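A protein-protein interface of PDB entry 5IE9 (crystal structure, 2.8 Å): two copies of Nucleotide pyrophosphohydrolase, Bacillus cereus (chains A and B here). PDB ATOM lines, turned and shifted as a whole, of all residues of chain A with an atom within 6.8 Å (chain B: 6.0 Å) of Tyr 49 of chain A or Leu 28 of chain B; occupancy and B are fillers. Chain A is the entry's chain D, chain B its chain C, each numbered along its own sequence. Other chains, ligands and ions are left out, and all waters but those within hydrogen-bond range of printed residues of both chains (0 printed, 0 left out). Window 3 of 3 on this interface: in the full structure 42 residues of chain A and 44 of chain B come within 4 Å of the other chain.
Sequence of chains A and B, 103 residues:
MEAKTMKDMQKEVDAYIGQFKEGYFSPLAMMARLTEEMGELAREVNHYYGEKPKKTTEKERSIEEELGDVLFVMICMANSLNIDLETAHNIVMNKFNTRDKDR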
ATOM      1  N   ALA A  42      -6.212 -20.328 -17.285  1.00  0.00           N
ATOM      2  CA  ALA A  42      -5.021 -20.292 -18.149  1.00  0.00           C
ATOM      3  C   ALA A  42      -4.125 -19.092 -17.862  1.00  0.00           C
ATOM      4  O   ALA A  42      -2.896 -19.249 -17.767  1.00  0.00           O
ATOM      5  CB  ALA A  42      -5.410 -20.321 -19.618  1.00  0.00           C
ATOM      6  N   GLU A  44      -3.930 -17.438 -15.022  1.00  0.00           N
ATOM      7  CA  GLU A  44      -3.320 -17.600 -13.705  1.00  0.00           C
ATOM      8  C   GLU A  44      -2.180 -18.617 -13.731  1.00  0.00           C
ATOM      9  O   GLU A  44      -1.120 -18.362 -13.167  1.00  0.00           O
ATOM     10  CB  GLU A  44      -4.366 -17.941 -12.643  1.00  0.00           C
ATOM     11  N   VAL A  45      -2.387 -19.742 -14.415  1.00  0.00           N
ATOM     12  CA  VAL A  45      -1.339 -20.760 -14.596  1.00  0.00           C
ATOM     13  C   VAL A  45      -0.106 -20.156 -15.284  1.00  0.00           C
ATOM     14  O   VAL A  45       1.004 -20.305 -14.778  1.00  0.00           O
ATOM     15  CB  VAL A  45      -1.860 -22.021 -15.339  1.00  0.00           C
ATOM     16  CG1 VAL A  45      -0.727 -22.980 -15.682  1.00  0.00           C
ATOM     17  CG2 VAL A  45      -2.911 -22.735 -14.502  1.00  0.00           C
ATOM     18  N   ASN A  46      -0.311 -19.453 -16.401  1.00  0.00           N
ATOM     19  CA  ASN A  46       0.777 -18.743 -17.095  1.00  0.00           C
ATOM     20  C   ASN A  46       1.524 -17.717 -16.219  1.00  0.00           C
ATOM     21  O   ASN A  46       2.750 -17.644 -16.265  1.00  0.00           O
ATOM     22  CB  ASN A  46       0.263 -18.068 -18.377  1.00  0.00           C
ATOM     23  CG  ASN A  46       1.231 -18.199 -19.553  1.00  0.00           C
ATOM     24  OD1 ASN A  46       0.825 -18.054 -20.705  1.00  0.00           O
ATOM     25  ND2 ASN A  46       2.506 -18.469 -19.275  1.00  0.00           N
ATOM     26  N   HIS A  47       0.773 -16.949 -15.426  1.00  0.00           N
ATOM     27  CA  HIS A  47       1.314 -15.946 -14.508  1.00  0.00           C
ATOM     28  C   HIS A  47       2.271 -16.577 -13.489  1.00  0.00           C
ATOM     29  O   HIS A  47       3.384 -16.088 -13.292  1.00  0.00           O
ATOM     30  CB  HIS A  47       0.162 -15.205 -13.805  1.00  0.00           C
ATOM     31  CG  HIS A  47       0.605 -14.142 -12.840  1.00  0.00           C
ATOM     32  ND1 HIS A  47       0.756 -14.378 -11.489  1.00  0.00           N
ATOM     33  CD2 HIS A  47       0.919 -12.837 -13.030  1.00  0.00           C
ATOM     34  CE1 HIS A  47       1.151 -13.268 -10.891  1.00  0.00           C
ATOM     35  NE2 HIS A  47       1.257 -12.317 -11.804  1.00  0.00           N
ATOM     36  N   TYR A  48       1.842 -17.675 -12.873  1.00  0.00           N
ATOM     37  CA  TYR A  48       2.608 -18.328 -11.815  1.00  0.00           C
ATOM     38  C   TYR A  48       3.607 -19.392 -12.294  1.00  0.00           C
ATOM     39  O   TYR A  48       4.514 -19.758 -11.541  1.00  0.00           O
ATOM     40  CB  TYR A  48       1.660 -18.934 -10.780  1.00  0.00           C
ATOM     41  CG  TYR A  48       0.977 -17.932  -9.873  1.00  0.00           C
ATOM     42  CD1 TYR A  48       1.593 -17.500  -8.684  1.00  0.00           C
ATOM     43  CD2 TYR A  48      -0.296 -17.430 -10.186  1.00  0.00           C
ATOM     44  CE1 TYR A  48       0.964 -16.589  -7.840  1.00  0.00           C
ATOM     45  CE2 TYR A  48      -0.934 -16.518  -9.349  1.00  0.00           C
ATOM     46  CZ  TYR A  48      -0.300 -16.101  -8.180  1.00  0.00           C
ATOM     47  OH  TYR A  48      -0.925 -15.202  -7.347  1.00  0.00           O
ATOM     48  N   TYR A  49       3.439 -19.891 -13.525  1.00  0.00           N
ATOM     49  CA  TYR A  49       4.271 -21.005 -14.040  1.00  0.00           C
ATOM     50  C   TYR A  49       4.864 -20.847 -15.458  1.00  0.00           C
ATOM     51  O   TYR A  49       5.472 -21.786 -15.990  1.00  0.00           O
ATOM     52  CB  TYR A  49       3.536 -22.345 -13.877  1.00  0.00           C
ATOM     53  CG  TYR A  49       3.120 -22.611 -12.443  1.00  0.00           C
ATOM     54  CD1 TYR A  49       4.052 -23.054 -11.486  1.00  0.00           C
ATOM     55  CD2 TYR A  49       1.800 -22.398 -12.029  1.00  0.00           C
ATOM     56  CE1 TYR A  49       3.672 -23.284 -10.167  1.00  0.00           C
ATOM     57  CE2 TYR A  49       1.415 -22.627 -10.716  1.00  0.00           C
ATOM     58  CZ  TYR A  49       2.348 -23.063  -9.791  1.00  0.00           C
ATOM     59  OH  TYR A  49       1.951 -23.284  -8.495  1.00  0.00           O
ATOM     60  N   GLY A  50       4.719 -19.652 -16.039  1.00  0.00           N
ATOM     61  CA  GLY A  50       5.301 -19.326 -17.344  1.00  0.00           C
ATOM     62  C   GLY A  50       6.768 -18.969 -17.249  1.00  0.00           C
ATOM     63  O   GLY A  50       7.386 -18.591 -18.243  1.00  0.00           O
ATOM     64  N   ILE A  63      -4.872 -19.365  -8.223  1.00  0.00           N
ATOM     65  CA  ILE A  63      -5.128 -20.620  -8.951  1.00  0.00           C
ATOM     66  C   ILE A  63      -6.207 -21.414  -8.225  1.00  0.00           C
ATOM     67  O   ILE A  63      -7.155 -21.876  -8.860  1.00  0.00           O
ATOM     68  CB  ILE A  63      -3.852 -21.462  -9.216  1.00  0.00           C
ATOM     69  CG1 ILE A  63      -2.918 -20.703 -10.158  1.00  0.00           C
ATOM     70  CG2 ILE A  63      -4.197 -22.801  -9.868  1.00  0.00           C
ATOM     71  CD1 ILE A  63      -1.506 -21.231 -10.203  1.00  0.00           C
ATOM     72  N   SER B  26       3.595 -31.134 -15.847  1.00  0.00           N
ATOM     73  CA  SER B  26       3.870 -29.754 -15.416  1.00  0.00           C
ATOM     74  C   SER B  26       2.624 -28.882 -15.629  1.00  0.00           C
ATOM     75  O   SER B  26       1.841 -29.157 -16.545  1.00  0.00           O
ATOM     76  CB  SER B  26       5.079 -29.176 -16.168  1.00  0.00           C
ATOM     77  OG  SER B  26       4.793 -28.941 -17.543  1.00  0.00           O
ATOM     78  N   PRO B  27       2.422 -27.843 -14.780  1.00  0.00           N
ATOM     79  CA  PRO B  27       1.190 -27.034 -14.843  1.00  0.00           C
ATOM     80  C   PRO B  27       0.800 -26.510 -16.240  1.00  0.00           C
ATOM     81  O   PRO B  27      -0.385 -26.483 -16.573  1.00  0.00           O
ATOM     82  CB  PRO B  27       1.466 -25.880 -13.862  1.00  0.00           C
ATOM     83  CG  PRO B  27       2.898 -26.006 -13.463  1.00  0.00           C
ATOM     84  CD  PRO B  27       3.257 -27.440 -13.636  1.00  0.00           C
ATOM     85  N   LEU B  28       1.785 -26.128 -17.050  1.00  0.00           N
ATOM     86  CA  LEU B  28       1.535 -25.635 -18.404  1.00  0.00           C
ATOM     87  C   LEU B  28       1.091 -26.757 -19.359  1.00  0.00           C
ATOM     88  O   LEU B  28       0.206 -26.550 -20.193  1.00  0.00           O
ATOM     89  CB  LEU B  28       2.778 -24.907 -18.919  1.00  0.00           C
ATOM     90  CG  LEU B  28       2.706 -23.542 -19.612  1.00  0.00           C
ATOM     91  CD1 LEU B  28       1.659 -22.609 -19.018  1.00  0.00           C
ATOM     92  CD2 LEU B  28       4.084 -22.894 -19.563  1.00  0.00           C
ATOM     93  N   ALA B  29       1.703 -27.934 -19.219  1.00  0.00           N
ATOM     94  CA  ALA B  29       1.273 -29.159 -19.907  1.00  0.00           C
ATOM     95  C   ALA B  29      -0.152 -29.583 -19.513  1.00  0.00           C
ATOM     96  O   ALA B  29      -0.937 -29.998 -20.373  1.00  0.00           O
ATOM     97  CB  ALA B  29       2.259 -30.284 -19.641  1.00  0.00           C
ATOM     98  N   MET B  30      -0.467 -29.475 -18.218  1.00  0.00           N
ATOM     99  CA  MET B  30      -1.819 -29.682 -17.679  1.00  0.00           C
ATOM    100  C   MET B  30      -2.827 -28.746 -18.307  1.00  0.00           C
ATOM    101  O   MET B  30      -3.946 -29.153 -18.615  1.00  0.00           O
ATOM    102  CB  MET B  30      -1.859 -29.406 -16.174  1.00  0.00           C
ATOM    103  CG  MET B  30      -1.163 -30.426 -15.314  1.00  0.00           C
ATOM    104  SD  MET B  30      -2.232 -31.831 -15.004  1.00  0.00           S
ATOM    105  CE  MET B  30      -1.289 -32.581 -13.675  1.00  0.00           C
ATOM    106  N   MET B  31      -2.436 -27.482 -18.462  1.00  0.00           N
ATOM    107  CA  MET B  31      -3.332 -26.476 -18.993  1.00  0.00           C
ATOM    108  C   MET B  31      -3.726 -26.832 -20.425  1.00  0.00           C
ATOM    109  O   MET B  31      -4.889 -26.654 -20.805  1.00  0.00           O
ATOM    110  CB  MET B  31      -2.722 -25.078 -18.878  1.00  0.00           C
ATOM    111  CG  MET B  31      -3.736 -23.948 -18.995  1.00  0.00           C
ATOM    112  SD  MET B  31      -5.113 -24.095 -17.838  1.00  0.00           S
ATOM    113  CE  MET B  31      -6.513 -23.789 -18.908  1.00  0.00           C
ATOM    114  N   ALA B  32      -2.764 -27.371 -21.188  1.00  0.00           N
ATOM    115  CA  ALA B  32      -3.004 -27.900 -22.529  1.00  0.00           C
ATOM    116  C   ALA B  32      -3.952 -29.095 -22.493  1.00  0.00           C
ATOM    117  O   ALA B  32      -4.889 -29.152 -23.299  1.00  0.00           O
ATOM    118  CB  ALA B  32      -1.697 -28.266 -23.205  1.00  0.00           C
ATOM    119  N   ARG B  33      -3.717 -30.024 -21.554  1.00  0.00           N
ATOM    120  CA  ARG B  33      -4.601 -31.177 -21.328  1.00  0.00           C
ATOM    121  C   ARG B  33      -6.049 -30.758 -21.087  1.00  0.00           C
ATOM    122  O   ARG B  33      -6.960 -31.315 -21.704  1.00  0.00           O
ATOM    123  CB  ARG B  33      -4.121 -32.076 -20.170  1.00  0.00           C
ATOM    124  CG  ARG B  33      -3.041 -33.121 -20.474  1.00  0.00           C
ATOM    125  CD  ARG B  33      -3.252 -34.011 -21.715  1.00  0.00           C
ATOM    126  NE  ARG B  33      -4.661 -34.308 -21.999  1.00  0.00           N
ATOM    127  CZ  ARG B  33      -5.362 -35.320 -21.496  1.00  0.00           C
ATOM    128  NH1 ARG B  33      -4.807 -36.199 -20.670  1.00  0.00           N
ATOM    129  NH2 ARG B  33      -6.635 -35.456 -21.836  1.00  0.00           N
ATOM    130  N   LEU B  81      -0.587 -29.216  -7.600  1.00  0.00           N
ATOM    131  CA  LEU B  81      -0.274 -27.959  -6.902  1.00  0.00           C
ATOM    132  C   LEU B  81      -0.746 -27.935  -5.441  1.00  0.00           C
ATOM    133  O   LEU B  81      -0.891 -26.863  -4.845  1.00  0.00           O
ATOM    134  CB  LEU B  81      -0.857 -26.759  -7.673  1.00  0.00           C
ATOM    135  CG  LEU B  81      -0.634 -26.639  -9.185  1.00  0.00           C
ATOM    136  CD1 LEU B  81      -1.624 -25.649  -9.779  1.00  0.00           C
ATOM    137  CD2 LEU B  81       0.797 -26.262  -9.538  1.00  0.00           C
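No position is printed for both chains.
Of the 6 pairs that touch across the chains among the printed residues, none has its exchanged pair printed and touching as well.
Of the printed residues of chain B, Tyr 49 of chain A touches Pro 27, Leu 28 and Leu 81.
Of the printed residues of chain A, Leu 28 of chain B touches Tyr 49 (3.99 Å).
Of the printed residues of chain A, Met 31 of chain B touches Ala 42.
Printed residues of chain B within 4 Å of Val 45 of chain A: Pro 27 (3.6 Å).
Printed residues of chain A within 4 Å of Leu 81 of chain B: Tyr 49 and Ile 63.
Printed residues of chain B within 4 Å of Ile 63 of chain A: Leu 81 (3.8 Å).
Gly 50 of chain A touches none of the printed residues of chain B.
The nearest printed residue of chain A that does not touch Leu 28 of chain B is Val 45 of chain A (4.1 Å).
The nearest printed residue of chain B that does not touch Ile 63 of chain A is Pro 27 of chain B (6.6 Å).
Among the printed residues, pairs that only touch across the chains: Ala 42 of chain A with Met 31 of chain B (3.7 Å), Val 45 of chain A with Pro 27 of chain B (3.6 Å), Tyr 49 of chain A with Pro 27 of chain B (3.6 Å), Tyr 49 of chain A with Leu 28 of chain B (3.99 Å), Tyr 49 of chain A with Leu 81 of chain B (3.4 Å) and Ile 63 of chain A with Leu 81 of chain B (3.8 Å).
Of the 9 printed residues of chain A, 4 touch a printed residue of chain B.
Hydrophobic or aromatic side chains of chain A that line the printed part of chain B: Ala 42, Val 45, Tyr 49 and Ile 63.
Of the 9 printed residues of chain B, 4 touch a printed residue of chain A.
Printed residues of chain B that touch a printed residue of chain A: Pro 27, Leu 28, Met 31 and Leu 81.
Hydrophobic or aromatic side chains of chain B within 4 Å of the printed part of chain A: Pro 27, Leu 28, Met 31 and Leu 81.
Among the printed residues, no Asp or Glu carboxylate lies within 4 Å of a Lys or Arg side-chain nitrogen of the other chain.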
